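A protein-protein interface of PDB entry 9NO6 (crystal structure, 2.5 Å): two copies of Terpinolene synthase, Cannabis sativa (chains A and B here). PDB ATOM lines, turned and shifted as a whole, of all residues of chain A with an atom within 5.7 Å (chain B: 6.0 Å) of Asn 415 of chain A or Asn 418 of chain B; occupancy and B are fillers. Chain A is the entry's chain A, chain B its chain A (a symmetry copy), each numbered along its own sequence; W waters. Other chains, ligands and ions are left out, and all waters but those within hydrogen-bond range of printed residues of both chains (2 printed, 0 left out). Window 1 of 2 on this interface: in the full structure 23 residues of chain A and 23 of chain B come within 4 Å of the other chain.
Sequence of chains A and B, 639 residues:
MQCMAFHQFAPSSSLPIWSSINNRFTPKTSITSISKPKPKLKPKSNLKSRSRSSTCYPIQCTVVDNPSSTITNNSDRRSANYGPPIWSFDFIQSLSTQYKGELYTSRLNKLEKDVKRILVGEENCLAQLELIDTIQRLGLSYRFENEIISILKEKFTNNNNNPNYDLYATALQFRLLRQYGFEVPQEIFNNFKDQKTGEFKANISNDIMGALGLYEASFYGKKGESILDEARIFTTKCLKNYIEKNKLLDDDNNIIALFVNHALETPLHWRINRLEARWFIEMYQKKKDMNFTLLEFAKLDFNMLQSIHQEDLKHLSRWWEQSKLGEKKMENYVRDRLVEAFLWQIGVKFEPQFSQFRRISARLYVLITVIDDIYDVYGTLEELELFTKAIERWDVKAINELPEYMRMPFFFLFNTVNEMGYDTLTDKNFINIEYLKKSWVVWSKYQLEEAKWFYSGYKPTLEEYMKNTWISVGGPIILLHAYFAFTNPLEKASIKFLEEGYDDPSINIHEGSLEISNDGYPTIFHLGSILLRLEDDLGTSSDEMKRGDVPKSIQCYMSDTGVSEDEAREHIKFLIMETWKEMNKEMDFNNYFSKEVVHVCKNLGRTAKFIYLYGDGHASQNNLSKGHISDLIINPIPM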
ATOM      1  N   VAL A 396     -23.001  13.489  10.983  1.00  0.00           N
ATOM      2  CA  VAL A 396     -22.239  12.246  10.945  1.00  0.00           C
ATOM      3  C   VAL A 396     -22.607  11.364   9.760  1.00  0.00           C
ATOM      4  O   VAL A 396     -21.921  10.367   9.507  1.00  0.00           O
ATOM      5  CB  VAL A 396     -22.427  11.478  12.269  1.00  0.00           C
ATOM      6  CG1 VAL A 396     -23.695  10.635  12.226  1.00  0.00           C
ATOM      7  CG2 VAL A 396     -21.201  10.628  12.581  1.00  0.00           C
ATOM      8  N   PHE A 410     -12.216  14.479   9.299  1.00  0.00           N
ATOM      9  CA  PHE A 410     -13.499  15.141   9.516  1.00  0.00           C
ATOM     10  C   PHE A 410     -14.256  14.516  10.677  1.00  0.00           C
ATOM     11  O   PHE A 410     -14.839  15.232  11.498  1.00  0.00           O
ATOM     12  CB  PHE A 410     -14.361  15.098   8.254  1.00  0.00           C
ATOM     13  CG  PHE A 410     -15.787  15.523   8.492  1.00  0.00           C
ATOM     14  CD1 PHE A 410     -16.132  16.865   8.497  1.00  0.00           C
ATOM     15  CD2 PHE A 410     -16.779  14.583   8.727  1.00  0.00           C
ATOM     16  CE1 PHE A 410     -17.437  17.260   8.724  1.00  0.00           C
ATOM     17  CE2 PHE A 410     -18.085  14.973   8.958  1.00  0.00           C
ATOM     18  CZ  PHE A 410     -18.415  16.312   8.954  1.00  0.00           C
ATOM     19  N   PHE A 411     -14.289  13.183  10.745  1.00  0.00           N
ATOM     20  CA  PHE A 411     -14.970  12.515  11.851  1.00  0.00           C
ATOM     21  C   PHE A 411     -14.340  12.898  13.184  1.00  0.00           C
ATOM     22  O   PHE A 411     -15.048  13.153  14.169  1.00  0.00           O
ATOM     23  CB  PHE A 411     -14.926  10.999  11.648  1.00  0.00           C
ATOM     24  CG  PHE A 411     -16.000  10.243  12.391  1.00  0.00           C
ATOM     25  CD1 PHE A 411     -16.861  10.890  13.263  1.00  0.00           C
ATOM     26  CD2 PHE A 411     -16.144   8.878  12.210  1.00  0.00           C
ATOM     27  CE1 PHE A 411     -17.841  10.188  13.942  1.00  0.00           C
ATOM     28  CE2 PHE A 411     -17.124   8.172  12.883  1.00  0.00           C
ATOM     29  CZ  PHE A 411     -17.972   8.828  13.751  1.00  0.00           C
ATOM     30  N   PHE A 412     -13.009  12.963  13.230  1.00  0.00           N
ATOM     31  CA  PHE A 412     -12.340  13.311  14.476  1.00  0.00           C
ATOM     32  C   PHE A 412     -12.605  14.761  14.865  1.00  0.00           C
ATOM     33  O   PHE A 412     -12.832  15.058  16.044  1.00  0.00           O
ATOM     34  CB  PHE A 412     -10.843  13.043  14.355  1.00  0.00           C
ATOM     35  CG  PHE A 412     -10.121  13.101  15.661  1.00  0.00           C
ATOM     36  CD1 PHE A 412     -10.518  12.298  16.717  1.00  0.00           C
ATOM     37  CD2 PHE A 412      -9.049  13.954  15.837  1.00  0.00           C
ATOM     38  CE1 PHE A 412      -9.863  12.347  17.926  1.00  0.00           C
ATOM     39  CE2 PHE A 412      -8.387  14.005  17.041  1.00  0.00           C
ATOM     40  CZ  PHE A 412      -8.798  13.203  18.091  1.00  0.00           C
ATOM     41  N   LEU A 413     -12.585  15.675  13.891  1.00  0.00           N
ATOM     42  CA  LEU A 413     -12.936  17.066  14.164  1.00  0.00           C
ATOM     43  C   LEU A 413     -14.367  17.183  14.674  1.00  0.00           C
ATOM     44  O   LEU A 413     -14.640  17.926  15.625  1.00  0.00           O
ATOM     45  CB  LEU A 413     -12.749  17.901  12.895  1.00  0.00           C
ATOM     46  CG  LEU A 413     -13.368  19.300  12.849  1.00  0.00           C
ATOM     47  CD1 LEU A 413     -12.607  20.257  13.747  1.00  0.00           C
ATOM     48  CD2 LEU A 413     -13.411  19.819  11.420  1.00  0.00           C
ATOM     49  N   PHE A 414     -15.291  16.457  14.042  1.00  0.00           N
ATOM     50  CA  PHE A 414     -16.684  16.431  14.472  1.00  0.00           C
ATOM     51  C   PHE A 414     -16.797  16.003  15.928  1.00  0.00           C
ATOM     52  O   PHE A 414     -17.405  16.703  16.751  1.00  0.00           O
ATOM     53  CB  PHE A 414     -17.463  15.485  13.550  1.00  0.00           C
ATOM     54  CG  PHE A 414     -18.927  15.369  13.864  1.00  0.00           C
ATOM     55  CD1 PHE A 414     -19.794  16.414  13.601  1.00  0.00           C
ATOM     56  CD2 PHE A 414     -19.443  14.187  14.374  1.00  0.00           C
ATOM     57  CE1 PHE A 414     -21.148  16.295  13.872  1.00  0.00           C
ATOM     58  CE2 PHE A 414     -20.793  14.062  14.645  1.00  0.00           C
ATOM     59  CZ  PHE A 414     -21.647  15.117  14.393  1.00  0.00           C
ATOM     60  N   ASN A 415     -16.195  14.861  16.270  1.00  0.00           N
ATOM     61  CA  ASN A 415     -16.280  14.359  17.638  1.00  0.00           C
ATOM     62  C   ASN A 415     -15.636  15.322  18.630  1.00  0.00           C
ATOM     63  O   ASN A 415     -16.188  15.569  19.708  1.00  0.00           O
ATOM     64  CB  ASN A 415     -15.634  12.977  17.734  1.00  0.00           C
ATOM     65  CG  ASN A 415     -16.424  11.913  16.999  1.00  0.00           C
ATOM     66  OD1 ASN A 415     -17.621  12.066  16.762  1.00  0.00           O
ATOM     67  ND2 ASN A 415     -15.756  10.826  16.637  1.00  0.00           N
ATOM     68  N   THR A 416     -14.481  15.893  18.278  1.00  0.00           N
ATOM     69  CA  THR A 416     -13.774  16.770  19.208  1.00  0.00           C
ATOM     70  C   THR A 416     -14.559  18.052  19.467  1.00  0.00           C
ATOM     71  O   THR A 416     -14.705  18.483  20.619  1.00  0.00           O
ATOM     72  CB  THR A 416     -12.382  17.092  18.663  1.00  0.00           C
ATOM     73  OG1 THR A 416     -11.738  15.880  18.247  1.00  0.00           O
ATOM     74  CG2 THR A 416     -11.534  17.766  19.730  1.00  0.00           C
ATOM     75  N   VAL A 417     -15.076  18.677  18.408  1.00  0.00           N
ATOM     76  CA  VAL A 417     -15.812  19.925  18.582  1.00  0.00           C
ATOM     77  C   VAL A 417     -17.131  19.674  19.304  1.00  0.00           C
ATOM     78  O   VAL A 417     -17.565  20.489  20.130  1.00  0.00           O
ATOM     79  CB  VAL A 417     -16.018  20.616  17.223  1.00  0.00           C
ATOM     80  CG1 VAL A 417     -16.947  21.809  17.363  1.00  0.00           C
ATOM     81  CG2 VAL A 417     -14.677  21.059  16.658  1.00  0.00           C
ATOM     82  N   ASN A 418     -17.785  18.541  19.029  1.00  0.00           N
ATOM     83  CA  ASN A 418     -18.983  18.211  19.791  1.00  0.00           C
ATOM     84  C   ASN A 418     -18.656  17.944  21.253  1.00  0.00           C
ATOM     85  O   ASN A 418     -19.464  18.254  22.135  1.00  0.00           O
ATOM     86  CB  ASN A 418     -19.690  17.010  19.170  1.00  0.00           C
ATOM     87  CG  ASN A 418     -20.192  17.294  17.772  1.00  0.00           C
ATOM     88  OD1 ASN A 418     -20.509  18.434  17.433  1.00  0.00           O
ATOM     89  ND2 ASN A 418     -20.260  16.258  16.949  1.00  0.00           N
ATOM     90  N   GLU A 419     -17.473  17.391  21.533  1.00  0.00           N
ATOM     91  CA  GLU A 419     -17.057  17.202  22.919  1.00  0.00           C
ATOM     92  C   GLU A 419     -16.838  18.542  23.611  1.00  0.00           C
ATOM     93  O   GLU A 419     -17.173  18.701  24.790  1.00  0.00           O
ATOM     94  CB  GLU A 419     -15.790  16.350  22.969  1.00  0.00           C
ATOM     95  CG  GLU A 419     -15.394  15.903  24.364  1.00  0.00           C
ATOM     96  CD  GLU A 419     -14.390  14.766  24.344  1.00  0.00           C
ATOM     97  OE1 GLU A 419     -13.671  14.624  23.331  1.00  0.00           O
ATOM     98  OE2 GLU A 419     -14.327  14.009  25.335  1.00  0.00           O
ATOM     99  N   MET A 420     -16.283  19.520  22.892  1.00  0.00           N
ATOM    100  CA  MET A 420     -16.143  20.860  23.462  1.00  0.00           C
ATOM    101  C   MET A 420     -17.507  21.494  23.724  1.00  0.00           C
ATOM    102  O   MET A 420     -17.717  22.141  24.762  1.00  0.00           O
ATOM    103  CB  MET A 420     -15.313  21.745  22.535  1.00  0.00           C
ATOM    104  CG  MET A 420     -13.984  21.139  22.120  1.00  0.00           C
ATOM    105  SD  MET A 420     -12.942  22.278  21.188  1.00  0.00           S
ATOM    106  CE  MET A 420     -14.133  23.525  20.704  1.00  0.00           C
ATOM    107  N   TRP B 394     -30.768  12.095  15.153  1.00  0.00           N
ATOM    108  CA  TRP B 394     -29.353  11.933  15.485  1.00  0.00           C
ATOM    109  C   TRP B 394     -28.526  13.095  14.935  1.00  0.00           C
ATOM    110  O   TRP B 394     -27.616  12.925  14.123  1.00  0.00           O
ATOM    111  CB  TRP B 394     -28.825  10.588  14.978  1.00  0.00           C
ATOM    112  CG  TRP B 394     -27.527  10.179  15.605  1.00  0.00           C
ATOM    113  CD1 TRP B 394     -26.273  10.418  15.125  1.00  0.00           C
ATOM    114  CD2 TRP B 394     -27.356   9.459  16.833  1.00  0.00           C
ATOM    115  NE1 TRP B 394     -25.332   9.892  15.977  1.00  0.00           N
ATOM    116  CE2 TRP B 394     -25.971   9.297  17.032  1.00  0.00           C
ATOM    117  CE3 TRP B 394     -28.240   8.935  17.781  1.00  0.00           C
ATOM    118  CZ2 TRP B 394     -25.449   8.635  18.141  1.00  0.00           C
ATOM    119  CZ3 TRP B 394     -27.719   8.276  18.881  1.00  0.00           C
ATOM    120  CH2 TRP B 394     -26.337   8.132  19.051  1.00  0.00           C
ATOM    121  N   LEU B 413     -24.836  10.790  25.062  1.00  0.00           N
ATOM    122  CA  LEU B 413     -25.027   9.576  24.272  1.00  0.00           C
ATOM    123  C   LEU B 413     -24.571   9.779  22.833  1.00  0.00           C
ATOM    124  O   LEU B 413     -23.911   8.908  22.250  1.00  0.00           O
ATOM    125  CB  LEU B 413     -26.499   9.162  24.315  1.00  0.00           C
ATOM    126  CG  LEU B 413     -26.993   8.128  23.301  1.00  0.00           C
ATOM    127  CD1 LEU B 413     -26.461   6.747  23.636  1.00  0.00           C
ATOM    128  CD2 LEU B 413     -28.513   8.121  23.239  1.00  0.00           C
ATOM    129  N   PHE B 414     -24.925  10.924  22.246  1.00  0.00           N
ATOM    130  CA  PHE B 414     -24.499  11.266  20.894  1.00  0.00           C
ATOM    131  C   PHE B 414     -22.981  11.234  20.776  1.00  0.00           C
ATOM    132  O   PHE B 414     -22.426  10.551  19.904  1.00  0.00           O
ATOM    133  CB  PHE B 414     -25.057  12.649  20.541  1.00  0.00           C
ATOM    134  CG  PHE B 414     -24.711  13.133  19.161  1.00  0.00           C
ATOM    135  CD1 PHE B 414     -25.292  12.562  18.043  1.00  0.00           C
ATOM    136  CD2 PHE B 414     -23.840  14.198  18.989  1.00  0.00           C
ATOM    137  CE1 PHE B 414     -24.986  13.023  16.774  1.00  0.00           C
ATOM    138  CE2 PHE B 414     -23.532  14.664  17.724  1.00  0.00           C
ATOM    139  CZ  PHE B 414     -24.107  14.077  16.615  1.00  0.00           C
ATOM    140  N   ASN B 415     -22.292  11.953  21.666  1.00  0.00           N
ATOM    141  CA  ASN B 415     -20.834  12.005  21.607  1.00  0.00           C
ATOM    142  C   ASN B 415     -20.215  10.629  21.820  1.00  0.00           C
ATOM    143  O   ASN B 415     -19.271  10.253  21.115  1.00  0.00           O
ATOM    144  CB  ASN B 415     -20.300  13.001  22.636  1.00  0.00           C
ATOM    145  CG  ASN B 415     -20.643  14.436  22.291  1.00  0.00           C
ATOM    146  OD1 ASN B 415     -20.907  14.762  21.135  1.00  0.00           O
ATOM    147  ND2 ASN B 415     -20.638  15.302  23.295  1.00  0.00           N
ATOM    148  N   THR B 416     -20.742   9.852  22.769  1.00  0.00           N
ATOM    149  CA  THR B 416     -20.154   8.551  23.075  1.00  0.00           C
ATOM    150  C   THR B 416     -20.319   7.580  21.911  1.00  0.00           C
ATOM    151  O   THR B 416     -19.368   6.885  21.525  1.00  0.00           O
ATOM    152  CB  THR B 416     -20.785   7.979  24.345  1.00  0.00           C
ATOM    153  OG1 THR B 416     -20.790   8.982  25.371  1.00  0.00           O
ATOM    154  CG2 THR B 416     -20.002   6.771  24.834  1.00  0.00           C
ATOM    155  N   VAL B 417     -21.519   7.517  21.332  1.00  0.00           N
ATOM    156  CA  VAL B 417     -21.754   6.587  20.232  1.00  0.00           C
ATOM    157  C   VAL B 417     -20.979   7.016  18.992  1.00  0.00           C
ATOM    158  O   VAL B 417     -20.459   6.173  18.248  1.00  0.00           O
ATOM    159  CB  VAL B 417     -23.262   6.457  19.957  1.00  0.00           C
ATOM    160  CG1 VAL B 417     -23.510   5.649  18.695  1.00  0.00           C
ATOM    161  CG2 VAL B 417     -23.951   5.802  21.143  1.00  0.00           C
ATOM    162  N   ASN B 418     -20.866   8.327  18.751  1.00  0.00           N
ATOM    163  CA  ASN B 418     -20.028   8.774  17.645  1.00  0.00           C
ATOM    164  C   ASN B 418     -18.561   8.454  17.894  1.00  0.00           C
ATOM    165  O   ASN B 418     -17.822   8.166  16.947  1.00  0.00           O
ATOM    166  CB  ASN B 418     -20.220  10.270  17.410  1.00  0.00           C
ATOM    167  CG  ASN B 418     -21.629  10.612  16.985  1.00  0.00           C
ATOM    168  OD1 ASN B 418     -22.318   9.802  16.365  1.00  0.00           O
ATOM    169  ND2 ASN B 418     -22.071  11.815  17.322  1.00  0.00           N
ATOM    170  N   GLU B 419     -18.126   8.477  19.156  1.00  0.00           N
ATOM    171  CA  GLU B 419     -16.758   8.081  19.471  1.00  0.00           C
ATOM    172  C   GLU B 419     -16.541   6.598  19.196  1.00  0.00           C
ATOM    173  O   GLU B 419     -15.475   6.201  18.714  1.00  0.00           O
ATOM    174  CB  GLU B 419     -16.444   8.416  20.929  1.00  0.00           C
ATOM    175  CG  GLU B 419     -14.982   8.255  21.305  1.00  0.00           C
ATOM    176  CD  GLU B 419     -14.641   8.950  22.608  1.00  0.00           C
ATOM    177  OE1 GLU B 419     -15.558   9.157  23.432  1.00  0.00           O
ATOM    178  OE2 GLU B 419     -13.457   9.299  22.805  1.00  0.00           O
ATOM    179  N   MET B 420     -17.543   5.767  19.489  1.00  0.00           N
ATOM    180  CA  MET B 420     -17.440   4.348  19.150  1.00  0.00           C
ATOM    181  C   MET B 420     -17.387   4.143  17.638  1.00  0.00           C
ATOM    182  O   MET B 420     -16.614   3.312  17.137  1.00  0.00           O
ATOM    183  CB  MET B 420     -18.611   3.574  19.752  1.00  0.00           C
ATOM    184  CG  MET B 420     -18.817   3.813  21.237  1.00  0.00           C
ATOM    185  SD  MET B 420     -20.078   2.745  21.961  1.00  0.00           S
ATOM    186  CE  MET B 420     -20.930   2.167  20.496  1.00  0.00           C
ATOM    187  N   GLY B 421     -18.211   4.885  16.897  1.00  0.00           N
ATOM    188  CA  GLY B 421     -18.151   4.814  15.445  1.00  0.00           C
ATOM    189  C   GLY B 421     -16.798   5.231  14.902  1.00  0.00           C
ATOM    190  O   GLY B 421     -16.283   4.629  13.955  1.00  0.00           O
ATOM    191  N   TYR B 422     -16.198   6.261  15.503  1.00  0.00           N
ATOM    192  CA  TYR B 422     -14.857   6.662  15.094  1.00  0.00           C
ATOM    193  C   TYR B 422     -13.830   5.598  15.452  1.00  0.00           C
ATOM    194  O   TYR B 422     -12.866   5.391  14.710  1.00  0.00           O
ATOM    195  CB  TYR B 422     -14.475   7.998  15.730  1.00  0.00           C
ATOM    196  CG  TYR B 422     -13.096   8.466  15.324  1.00  0.00           C
ATOM    197  CD1 TYR B 422     -12.899   9.148  14.131  1.00  0.00           C
ATOM    198  CD2 TYR B 422     -11.988   8.213  16.123  1.00  0.00           C
ATOM    199  CE1 TYR B 422     -11.643   9.572  13.749  1.00  0.00           C
ATOM    200  CE2 TYR B 422     -10.725   8.632  15.749  1.00  0.00           C
ATOM    201  CZ  TYR B 422     -10.559   9.312  14.560  1.00  0.00           C
ATOM    202  OH  TYR B 422      -9.307   9.735  14.177  1.00  0.00           O
ATOM    203  N   ASP B 423     -14.006   4.932  16.596  1.00  0.00           N
ATOM    204  CA  ASP B 423     -13.126   3.821  16.943  1.00  0.00           C
ATOM    205  C   ASP B 423     -13.179   2.735  15.880  1.00  0.00           C
ATOM    206  O   ASP B 423     -12.145   2.173  15.498  1.00  0.00           O
ATOM    207  CB  ASP B 423     -13.504   3.249  18.311  1.00  0.00           C
ATOM    208  CG  ASP B 423     -12.975   4.082  19.458  1.00  0.00           C
ATOM    209  OD1 ASP B 423     -11.921   4.731  19.288  1.00  0.00           O
ATOM    210  OD2 ASP B 423     -13.610   4.084  20.535  1.00  0.00           O
ATOM    211  N   ILE B 433     -21.413   3.939  11.980  1.00  0.00           N
ATOM    212  CA  ILE B 433     -22.236   4.841  12.782  1.00  0.00           C
ATOM    213  C   ILE B 433     -23.700   4.731  12.384  1.00  0.00           C
ATOM    214  O   ILE B 433     -24.596   4.929  13.216  1.00  0.00           O
ATOM    215  CB  ILE B 433     -21.716   6.289  12.661  1.00  0.00           C
ATOM    216  CG1 ILE B 433     -22.443   7.202  13.648  1.00  0.00           C
ATOM    217  CG2 ILE B 433     -21.868   6.806  11.236  1.00  0.00           C
ATOM    218  CD1 ILE B 433     -22.325   6.753  15.087  1.00  0.00           C
HETATM  219  O   HOH W   1     -17.794  12.932  20.350  1.00  0.00           O
HETATM  220  O   HOH W   2     -19.970  13.645  18.276  1.00  0.00           O
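O of Asn 418 of chain B lies within hydrogen-bond range of ND2 of Asn 415 of chain A, at 3.4 Å.
The backbone carbonyl oxygen (O) of Asn 418 of chain A is in hydrogen-bond range of the side-chain amide nitrogen (ND2) of Asn 415 of chain B, at 3.4 Å.
The backbone carbonyl oxygen (O) of Phe 411 of chain A lies close to the side-chain amide nitrogen (ND2) of Asn 415 of chain A.
OG1 of Thr 416 of chain A is in hydrogen-bond range of O of Phe 412 of chain A, 2.6 Å away.
ND2 of Asn 418 of chain A sits at hydrogen-bond distance from O of Phe 414 of chain A, 2.9 Å away.
NE1 of Trp 394 of chain B lies within hydrogen-bond range of OD1 of Asn 418 of chain B (3.0 Å).
The side-chain amide nitrogen (ND2) of Asn 418 of chain B is in hydrogen-bond range of the backbone carbonyl oxygen (O) of Phe 414 of chain B (2.9 Å).
Among the printed residues, merely in contact across the chains: Asn 415 of chain A with Tyr 422 of chain B (3.2 Å), Phe 411 of chain A with Asn 418 of chain B (3.3 Å), Phe 411 of chain A with Tyr 422 of chain B (3.4 Å), Phe 414 of chain A with Phe 414 of chain B (3.5 Å), Phe 411 of chain A with Gly 421 of chain B (3.6 Å), Phe 412 of chain A with Tyr 422 of chain B (3.6 Å), Asn 418 of chain A with Phe 414 of chain B (3.7 Å), Phe 414 of chain A with Asn 418 of chain B (3.7 Å), Val 396 of chain A with Ile 433 of chain B (3.8 Å) and Val 396 of chain A with Trp 394 of chain B (3.9 Å).
Printed residues of chain B within 4 Å of Phe 411 of chain A: Asn 418, Gly 421 and Tyr 422.
Of the printed residues of chain B, Phe 412 of chain A touches Tyr 422 (3.6 Å).
Printed residues of chain B within 4 Å of Phe 414 of chain A: Phe 414 (3.5 Å) and Asn 418 (3.7 Å).
Printed residues of chain B within 4 Å of Asn 415 of chain A: Asn 418 (3.2 Å) and Tyr 422 (3.2 Å).
Printed residues of chain B within 4 Å of Asn 418 of chain A: Phe 414 (3.7 Å) and Asn 415 (3.2 Å).
Asn 418 of chain B touches three residues of chain A.
The nearest residue of chain B that does not touch Asn 415 of chain A is Glu 419 of chain B (4.1 Å).
Printed residues of chain A that touch a printed residue of chain B: Val 396, Phe 411, Phe 412, Phe 414, Asn 415 and Asn 418.
Hydrophobic or aromatic side chains of chain B that line the printed part of chain A: Trp 394, Phe 414, Tyr 422 and Ile 433.
Among the printed residues, no Asp or Glu carboxylate lies within 4 Å of a Lys or Arg side-chain nitrogen of the other chain.
Phe 414 of chain A touches its own counterpart, Phe 414 of chain B.
Phe 414 of chain A touches Asn 418 of chain B, and with the chains exchanged Asn 418 of chain A touches Phe 414 of chain B.
Asn 415 of chain A touches Asn 418 of chain B, and with the chains exchanged Asn 418 of chain A touches Asn 415 of chain B.
Water W2 lies within hydrogen-bond range of ND2 of Asn 418 of chain A (2.9 Å), ND2 of Asn 418 of chain B (2.9 Å), OD1 of Asn 415 of chain A (3.2 Å) and OD1 of Asn 415 of chain B (3.2 Å).
Water W1 lies within hydrogen-bond range of O of Asn 415 of chain A and O of Asn 415 of chain B.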
